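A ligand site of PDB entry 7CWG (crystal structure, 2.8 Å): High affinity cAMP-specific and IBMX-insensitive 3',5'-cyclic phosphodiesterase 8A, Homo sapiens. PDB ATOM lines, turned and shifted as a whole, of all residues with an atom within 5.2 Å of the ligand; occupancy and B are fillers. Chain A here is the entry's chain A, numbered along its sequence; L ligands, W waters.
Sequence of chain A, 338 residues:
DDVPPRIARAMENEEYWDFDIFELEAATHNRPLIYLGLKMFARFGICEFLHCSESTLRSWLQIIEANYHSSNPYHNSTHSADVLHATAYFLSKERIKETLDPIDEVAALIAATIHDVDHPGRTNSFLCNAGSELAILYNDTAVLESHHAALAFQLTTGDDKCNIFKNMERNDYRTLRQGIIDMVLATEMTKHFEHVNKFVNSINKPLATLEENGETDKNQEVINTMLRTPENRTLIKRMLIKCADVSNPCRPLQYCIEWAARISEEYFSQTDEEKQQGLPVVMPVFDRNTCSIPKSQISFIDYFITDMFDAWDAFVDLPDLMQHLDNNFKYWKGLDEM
ND2 of Asn 248 sits at hydrogen-bond distance from OH of Tyr 74, at 3.0 Å.
SD of Met 189 touches C8 of the ligand, at 3.9 Å. His 192 touches the ligand. Lys 242 touches the ligand (NZ to F1, 3.9 Å). Val 246 touches the ligand (CG2 to F2, 3.7 Å). Ile 263 touches the ligand. Phe 286 touches the ligand (CE2 to CL1, 3.6 Å). Phe 300 touches the ligand (CE2 to C4, 3.3 Å). Phe 304 touches the ligand. Met 308 touches the ligand. Hydrophobic or aromatic side chains that line the ligand: Tyr 74, Met 189, His 192, Val 246, Ile 263, Tyr 267, Phe 286, Phe 300, Phe 304 and Met 308. 13 residues have an atom within 4 Å of the ligand: Tyr 74, Met 189, His 192, Lys 242, Val 246, Asn 248, Ile 263, Tyr 267, Phe 286, Gln 297, Phe 300, Phe 304 and Met 308.
Water W2 bridges O of Asp 245 and OH of Tyr 74. Water W3 bridges NE2 of His 75 (3.2 Å) and OD2 of Asp 245 (3.5 Å).
The side-chain hydroxyl of Tyr 267 lies within hydrogen-bond range of a nitrogen (N6) of the ligand. N5 of the ligand is in hydrogen-bond range of OD1 of Asn 248, at 2.9 Å. A nitrogen (N4) of the ligand lies close to the side-chain hydroxyl (OH) of Tyr 74 (3.4 Å). The side-chain amide nitrogen of Gln 297 is in hydrogen-bond range of a nitrogen (N1) of the ligand, 3.5 Å away.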
ATOM      1  N   TYR A  74       7.645  16.324  18.774  1.00  0.00           N
ATOM      2  CA  TYR A  74       6.879  16.839  19.916  1.00  0.00           C
ATOM      3  C   TYR A  74       7.068  15.992  21.165  1.00  0.00           C
ATOM      4  O   TYR A  74       7.569  16.474  22.180  1.00  0.00           O
ATOM      5  CB  TYR A  74       5.390  16.908  19.548  1.00  0.00           C
ATOM      6  CG  TYR A  74       4.490  17.532  20.586  1.00  0.00           C
ATOM      7  CD1 TYR A  74       4.271  18.903  20.614  1.00  0.00           C
ATOM      8  CD2 TYR A  74       3.837  16.738  21.528  1.00  0.00           C
ATOM      9  CE1 TYR A  74       3.427  19.475  21.558  1.00  0.00           C
ATOM     10  CE2 TYR A  74       2.998  17.296  22.481  1.00  0.00           C
ATOM     11  CZ  TYR A  74       2.786  18.662  22.497  1.00  0.00           C
ATOM     12  OH  TYR A  74       1.952  19.215  23.429  1.00  0.00           O
ATOM     13  N   HIS A  75       6.676  14.721  21.079  1.00  0.00           N
ATOM     14  CA  HIS A  75       6.638  13.831  22.252  1.00  0.00           C
ATOM     15  C   HIS A  75       8.034  13.331  22.625  1.00  0.00           C
ATOM     16  O   HIS A  75       8.424  12.203  22.309  1.00  0.00           O
ATOM     17  CB  HIS A  75       5.650  12.668  22.044  1.00  0.00           C
ATOM     18  CG  HIS A  75       4.222  13.048  22.238  1.00  0.00           C
ATOM     19  ND1 HIS A  75       3.310  13.100  21.211  1.00  0.00           N
ATOM     20  CD2 HIS A  75       3.550  13.406  23.359  1.00  0.00           C
ATOM     21  CE1 HIS A  75       2.132  13.464  21.690  1.00  0.00           C
ATOM     22  NE2 HIS A  75       2.247  13.659  22.985  1.00  0.00           N
ATOM     23  N   THR A 187      -5.037  11.796  30.857  1.00  0.00           N
ATOM     24  CA  THR A 187      -4.542  12.526  29.671  1.00  0.00           C
ATOM     25  C   THR A 187      -5.120  12.075  28.315  1.00  0.00           C
ATOM     26  O   THR A 187      -4.863  12.735  27.299  1.00  0.00           O
ATOM     27  CB  THR A 187      -3.000  12.427  29.589  1.00  0.00           C
ATOM     28  OG1 THR A 187      -2.610  11.052  29.557  1.00  0.00           O
ATOM     29  CG2 THR A 187      -2.348  13.108  30.790  1.00  0.00           C
ATOM     30  N   MET A 189      -7.493  11.431  25.068  1.00  0.00           N
ATOM     31  CA  MET A 189      -8.366  12.323  24.286  1.00  0.00           C
ATOM     32  C   MET A 189      -9.853  11.990  24.464  1.00  0.00           C
ATOM     33  O   MET A 189     -10.631  12.867  24.837  1.00  0.00           O
ATOM     34  CB  MET A 189      -8.000  12.244  22.791  1.00  0.00           C
ATOM     35  CG  MET A 189      -8.800  13.187  21.883  1.00  0.00           C
ATOM     36  SD  MET A 189      -8.399  13.017  20.135  1.00  0.00           S
ATOM     37  CE  MET A 189      -9.675  14.031  19.386  1.00  0.00           C
ATOM     38  N   HIS A 192     -12.276  13.659  26.998  1.00  0.00           N
ATOM     39  CA  HIS A 192     -12.055  15.104  27.192  1.00  0.00           C
ATOM     40  C   HIS A 192     -13.303  15.779  27.771  1.00  0.00           C
ATOM     41  O   HIS A 192     -13.264  16.296  28.891  1.00  0.00           O
ATOM     42  CB  HIS A 192     -11.648  15.788  25.881  1.00  0.00           C
ATOM     43  CG  HIS A 192     -11.714  17.296  25.930  1.00  0.00           C
ATOM     44  ND1 HIS A 192     -10.779  18.053  26.594  1.00  0.00           N
ATOM     45  CD2 HIS A 192     -12.612  18.162  25.429  1.00  0.00           C
ATOM     46  CE1 HIS A 192     -11.089  19.335  26.487  1.00  0.00           C
ATOM     47  NE2 HIS A 192     -12.203  19.427  25.776  1.00  0.00           N
ATOM     48  N   LYS A 242      -4.539  17.735  32.582  1.00  0.00           N
ATOM     49  CA  LYS A 242      -5.053  17.935  31.209  1.00  0.00           C
ATOM     50  C   LYS A 242      -4.719  19.321  30.654  1.00  0.00           C
ATOM     51  O   LYS A 242      -4.366  19.444  29.491  1.00  0.00           O
ATOM     52  CB  LYS A 242      -6.556  17.687  31.136  1.00  0.00           C
ATOM     53  CG  LYS A 242      -6.937  16.210  31.219  1.00  0.00           C
ATOM     54  CD  LYS A 242      -8.441  15.993  31.331  1.00  0.00           C
ATOM     55  CE  LYS A 242      -9.205  16.518  30.115  1.00  0.00           C
ATOM     56  NZ  LYS A 242      -8.605  16.056  28.823  1.00  0.00           N
ATOM     57  N   ASP A 245      -0.901  19.474  30.028  1.00  0.00           N
ATOM     58  CA  ASP A 245      -0.584  18.686  28.832  1.00  0.00           C
ATOM     59  C   ASP A 245      -0.758  19.460  27.518  1.00  0.00           C
ATOM     60  O   ASP A 245       0.007  19.242  26.573  1.00  0.00           O
ATOM     61  CB  ASP A 245      -1.424  17.391  28.797  1.00  0.00           C
ATOM     62  CG  ASP A 245      -0.949  16.393  27.750  1.00  0.00           C
ATOM     63  OD1 ASP A 245       0.279  16.197  27.609  1.00  0.00           O
ATOM     64  OD2 ASP A 245      -1.807  15.776  27.072  1.00  0.00           O
ATOM     65  N   VAL A 246      -1.735  20.370  27.472  1.00  0.00           N
ATOM     66  CA  VAL A 246      -2.016  21.181  26.272  1.00  0.00           C
ATOM     67  C   VAL A 246      -2.008  22.684  26.572  1.00  0.00           C
ATOM     68  O   VAL A 246      -2.908  23.434  26.161  1.00  0.00           O
ATOM     69  CB  VAL A 246      -3.342  20.751  25.590  1.00  0.00           C
ATOM     70  CG1 VAL A 246      -3.199  19.343  25.025  1.00  0.00           C
ATOM     71  CG2 VAL A 246      -4.531  20.815  26.548  1.00  0.00           C
ATOM     72  N   ASN A 248       0.391  24.749  25.479  1.00  0.00           N
ATOM     73  CA  ASN A 248       1.195  25.428  24.454  1.00  0.00           C
ATOM     74  C   ASN A 248       0.490  26.545  23.640  1.00  0.00           C
ATOM     75  O   ASN A 248       1.143  27.509  23.240  1.00  0.00           O
ATOM     76  CB  ASN A 248       1.986  24.465  23.537  1.00  0.00           C
ATOM     77  CG  ASN A 248       1.149  23.341  22.941  1.00  0.00           C
ATOM     78  OD1 ASN A 248       0.421  23.528  21.980  1.00  0.00           O
ATOM     79  ND2 ASN A 248       1.294  22.138  23.502  1.00  0.00           N
ATOM     80  N   PRO A 249      -0.844  26.429  23.401  1.00  0.00           N
ATOM     81  CA  PRO A 249      -1.546  27.608  22.873  1.00  0.00           C
ATOM     82  C   PRO A 249      -1.597  28.841  23.794  1.00  0.00           C
ATOM     83  O   PRO A 249      -1.803  29.948  23.317  1.00  0.00           O
ATOM     84  CB  PRO A 249      -2.977  27.084  22.609  1.00  0.00           C
ATOM     85  CG  PRO A 249      -3.055  25.780  23.326  1.00  0.00           C
ATOM     86  CD  PRO A 249      -1.682  25.228  23.285  1.00  0.00           C
ATOM     87  N   ALA A 260       3.371  24.127  17.911  1.00  0.00           N
ATOM     88  CA  ALA A 260       2.396  23.810  16.862  1.00  0.00           C
ATOM     89  C   ALA A 260       3.034  23.087  15.683  1.00  0.00           C
ATOM     90  O   ALA A 260       2.456  22.148  15.149  1.00  0.00           O
ATOM     91  CB  ALA A 260       1.706  25.078  16.373  1.00  0.00           C
ATOM     92  N   ILE A 263       4.135  19.225  16.868  1.00  0.00           N
ATOM     93  CA  ILE A 263       3.001  18.289  16.856  1.00  0.00           C
ATOM     94  C   ILE A 263       2.411  18.125  15.444  1.00  0.00           C
ATOM     95  O   ILE A 263       1.973  17.035  15.093  1.00  0.00           O
ATOM     96  CB  ILE A 263       1.891  18.671  17.883  1.00  0.00           C
ATOM     97  CG1 ILE A 263       0.888  17.523  18.066  1.00  0.00           C
ATOM     98  CG2 ILE A 263       1.162  19.959  17.494  1.00  0.00           C
ATOM     99  CD1 ILE A 263       1.480  16.214  18.534  1.00  0.00           C
ATOM    100  N   TYR A 267       2.016  14.478  13.384  1.00  0.00           N
ATOM    101  CA  TYR A 267       0.787  14.021  12.733  1.00  0.00           C
ATOM    102  C   TYR A 267       0.952  13.799  11.227  1.00  0.00           C
ATOM    103  O   TYR A 267       0.315  12.911  10.664  1.00  0.00           O
ATOM    104  CB  TYR A 267      -0.394  14.962  13.025  1.00  0.00           C
ATOM    105  CG  TYR A 267      -0.946  14.848  14.433  1.00  0.00           C
ATOM    106  CD1 TYR A 267      -1.170  13.600  15.028  1.00  0.00           C
ATOM    107  CD2 TYR A 267      -1.286  15.992  15.168  1.00  0.00           C
ATOM    108  CE1 TYR A 267      -1.682  13.485  16.305  1.00  0.00           C
ATOM    109  CE2 TYR A 267      -1.806  15.881  16.447  1.00  0.00           C
ATOM    110  CZ  TYR A 267      -2.006  14.627  17.006  1.00  0.00           C
ATOM    111  OH  TYR A 267      -2.508  14.471  18.271  1.00  0.00           O
ATOM    112  N   PHE A 286      -4.767  16.230   8.880  1.00  0.00           N
ATOM    113  CA  PHE A 286      -3.350  16.437   9.215  1.00  0.00           C
ATOM    114  C   PHE A 286      -2.433  15.750   8.204  1.00  0.00           C
ATOM    115  O   PHE A 286      -1.793  14.744   8.522  1.00  0.00           O
ATOM    116  CB  PHE A 286      -3.064  15.944  10.631  1.00  0.00           C
ATOM    117  CG  PHE A 286      -3.882  16.617  11.704  1.00  0.00           C
ATOM    118  CD1 PHE A 286      -5.131  16.124  12.057  1.00  0.00           C
ATOM    119  CD2 PHE A 286      -3.396  17.744  12.351  1.00  0.00           C
ATOM    120  CE1 PHE A 286      -5.882  16.741  13.043  1.00  0.00           C
ATOM    121  CE2 PHE A 286      -4.151  18.374  13.339  1.00  0.00           C
ATOM    122  CZ  PHE A 286      -5.398  17.868  13.680  1.00  0.00           C
ATOM    123  N   GLN A 297      -4.684  25.096  13.935  1.00  0.00           N
ATOM    124  CA  GLN A 297      -4.491  25.633  15.289  1.00  0.00           C
ATOM    125  C   GLN A 297      -5.703  26.441  15.790  1.00  0.00           C
ATOM    126  O   GLN A 297      -6.056  26.354  16.964  1.00  0.00           O
ATOM    127  CB  GLN A 297      -3.221  26.478  15.364  1.00  0.00           C
ATOM    128  CG  GLN A 297      -1.934  25.661  15.297  1.00  0.00           C
ATOM    129  CD  GLN A 297      -1.756  24.734  16.486  1.00  0.00           C
ATOM    130  OE1 GLN A 297      -2.111  25.090  17.614  1.00  0.00           O
ATOM    131  NE2 GLN A 297      -1.206  23.549  16.249  1.00  0.00           N
ATOM    132  N   PHE A 300      -8.210  23.710  16.510  1.00  0.00           N
ATOM    133  CA  PHE A 300      -7.745  23.066  17.746  1.00  0.00           C
ATOM    134  C   PHE A 300      -8.135  23.875  18.977  1.00  0.00           C
ATOM    135  O   PHE A 300      -8.681  23.323  19.941  1.00  0.00           O
ATOM    136  CB  PHE A 300      -6.224  22.856  17.698  1.00  0.00           C
ATOM    137  CG  PHE A 300      -5.665  22.207  18.945  1.00  0.00           C
ATOM    138  CD1 PHE A 300      -5.820  20.848  19.167  1.00  0.00           C
ATOM    139  CD2 PHE A 300      -4.987  22.962  19.896  1.00  0.00           C
ATOM    140  CE1 PHE A 300      -5.311  20.251  20.312  1.00  0.00           C
ATOM    141  CE2 PHE A 300      -4.482  22.378  21.042  1.00  0.00           C
ATOM    142  CZ  PHE A 300      -4.644  21.011  21.255  1.00  0.00           C
ATOM    143  N   PHE A 304     -11.378  22.320  21.523  1.00  0.00           N
ATOM    144  CA  PHE A 304     -10.945  21.743  22.807  1.00  0.00           C
ATOM    145  C   PHE A 304     -10.500  22.774  23.849  1.00  0.00           C
ATOM    146  O   PHE A 304     -11.030  22.811  24.958  1.00  0.00           O
ATOM    147  CB  PHE A 304      -9.796  20.768  22.572  1.00  0.00           C
ATOM    148  CG  PHE A 304     -10.142  19.638  21.651  1.00  0.00           C
ATOM    149  CD1 PHE A 304      -9.826  19.705  20.301  1.00  0.00           C
ATOM    150  CD2 PHE A 304     -10.779  18.490  22.127  1.00  0.00           C
ATOM    151  CE1 PHE A 304     -10.140  18.655  19.436  1.00  0.00           C
ATOM    152  CE2 PHE A 304     -11.097  17.445  21.283  1.00  0.00           C
ATOM    153  CZ  PHE A 304     -10.771  17.529  19.932  1.00  0.00           C
ATOM    154  N   ILE A 305      -9.530  23.611  23.465  1.00  0.00           N
ATOM    155  CA  ILE A 305      -8.771  24.425  24.421  1.00  0.00           C
ATOM    156  C   ILE A 305      -9.629  25.495  25.118  1.00  0.00           C
ATOM    157  O   ILE A 305      -9.658  25.545  26.349  1.00  0.00           O
ATOM    158  CB  ILE A 305      -7.538  25.098  23.726  1.00  0.00           C
ATOM    159  CG1 ILE A 305      -6.557  24.054  23.158  1.00  0.00           C
ATOM    160  CG2 ILE A 305      -6.793  26.034  24.676  1.00  0.00           C
ATOM    161  CD1 ILE A 305      -5.739  23.299  24.197  1.00  0.00           C
ATOM    162  N   MET A 308     -12.045  24.545  27.838  1.00  0.00           N
ATOM    163  CA  MET A 308     -11.316  23.865  28.917  1.00  0.00           C
ATOM    164  C   MET A 308     -10.627  24.885  29.817  1.00  0.00           C
ATOM    165  O   MET A 308     -10.801  24.865  31.047  1.00  0.00           O
ATOM    166  CB  MET A 308     -10.272  22.890  28.346  1.00  0.00           C
ATOM    167  CG  MET A 308      -9.865  21.778  29.293  1.00  0.00           C
ATOM    168  SD  MET A 308      -8.141  21.241  29.149  1.00  0.00           S
ATOM    169  CE  MET A 308      -7.856  21.247  27.376  1.00  0.00           C
HETATM  170  N1  LIG L   1      -2.330  21.089  18.414  1.00  0.00           N
HETATM  171  C1  LIG L   1      -2.726  19.849  18.166  1.00  0.00           C
HETATM  172  N2  LIG L   1      -2.592  18.737  18.872  1.00  0.00           N
HETATM  173  C2  LIG L   1      -1.944  18.979  20.018  1.00  0.00           C
HETATM  174  C3  LIG L   1      -1.448  20.204  20.440  1.00  0.00           C
HETATM  175  C4  LIG L   1      -1.675  21.295  19.578  1.00  0.00           C
HETATM  176  N3  LIG L   1      -1.612  18.085  21.013  1.00  0.00           N
HETATM  177  C5  LIG L   1      -0.957  18.819  21.968  1.00  0.00           C
HETATM  178  N4  LIG L   1      -0.822  20.089  21.668  1.00  0.00           N
HETATM  179  N5  LIG L   1      -1.278  22.547  19.847  1.00  0.00           N
HETATM  180 CL1  LIG L   1      -3.587  19.653  16.666  1.00  0.00          CL
HETATM  181  C6  LIG L   1      -1.907  16.630  20.997  1.00  0.00           C
HETATM  182  C7  LIG L   1      -3.396  16.387  21.146  1.00  0.00           C
HETATM  183  N6  LIG L   1      -3.924  15.480  20.316  1.00  0.00           N
HETATM  184  C8  LIG L   1      -5.254  15.278  20.382  1.00  0.00           C
HETATM  185  C9  LIG L   1      -6.085  15.939  21.263  1.00  0.00           C
HETATM  186  C10 LIG L   1      -5.517  16.861  22.126  1.00  0.00           C
HETATM  187  C11 LIG L   1      -4.155  17.093  22.075  1.00  0.00           C
HETATM  188  O1  LIG L   1      -6.132  17.628  23.077  1.00  0.00           O
HETATM  189  C12 LIG L   1      -7.554  17.564  23.224  1.00  0.00           C
HETATM  190  C13 LIG L   1      -7.737  17.832  24.744  1.00  0.00           C
HETATM  191  F1  LIG L   1      -6.892  17.053  25.472  1.00  0.00           F
HETATM  192  F2  LIG L   1      -7.400  19.118  25.025  1.00  0.00           F
HETATM  193  C14 LIG L   1      -1.131  15.904  22.097  1.00  0.00           C
HETATM  194  O   HOH W   1      -6.272  16.716  17.431  1.00  0.00           O
HETATM  195  O   HOH W   2       0.494  16.910  24.755  1.00  0.00           O
HETATM  196  O   HOH W   3      -0.468  13.713  24.623  1.00  0.00           O
HETATM  197  O   HOH W   4      -4.132  12.615  21.534  1.00  0.00           O
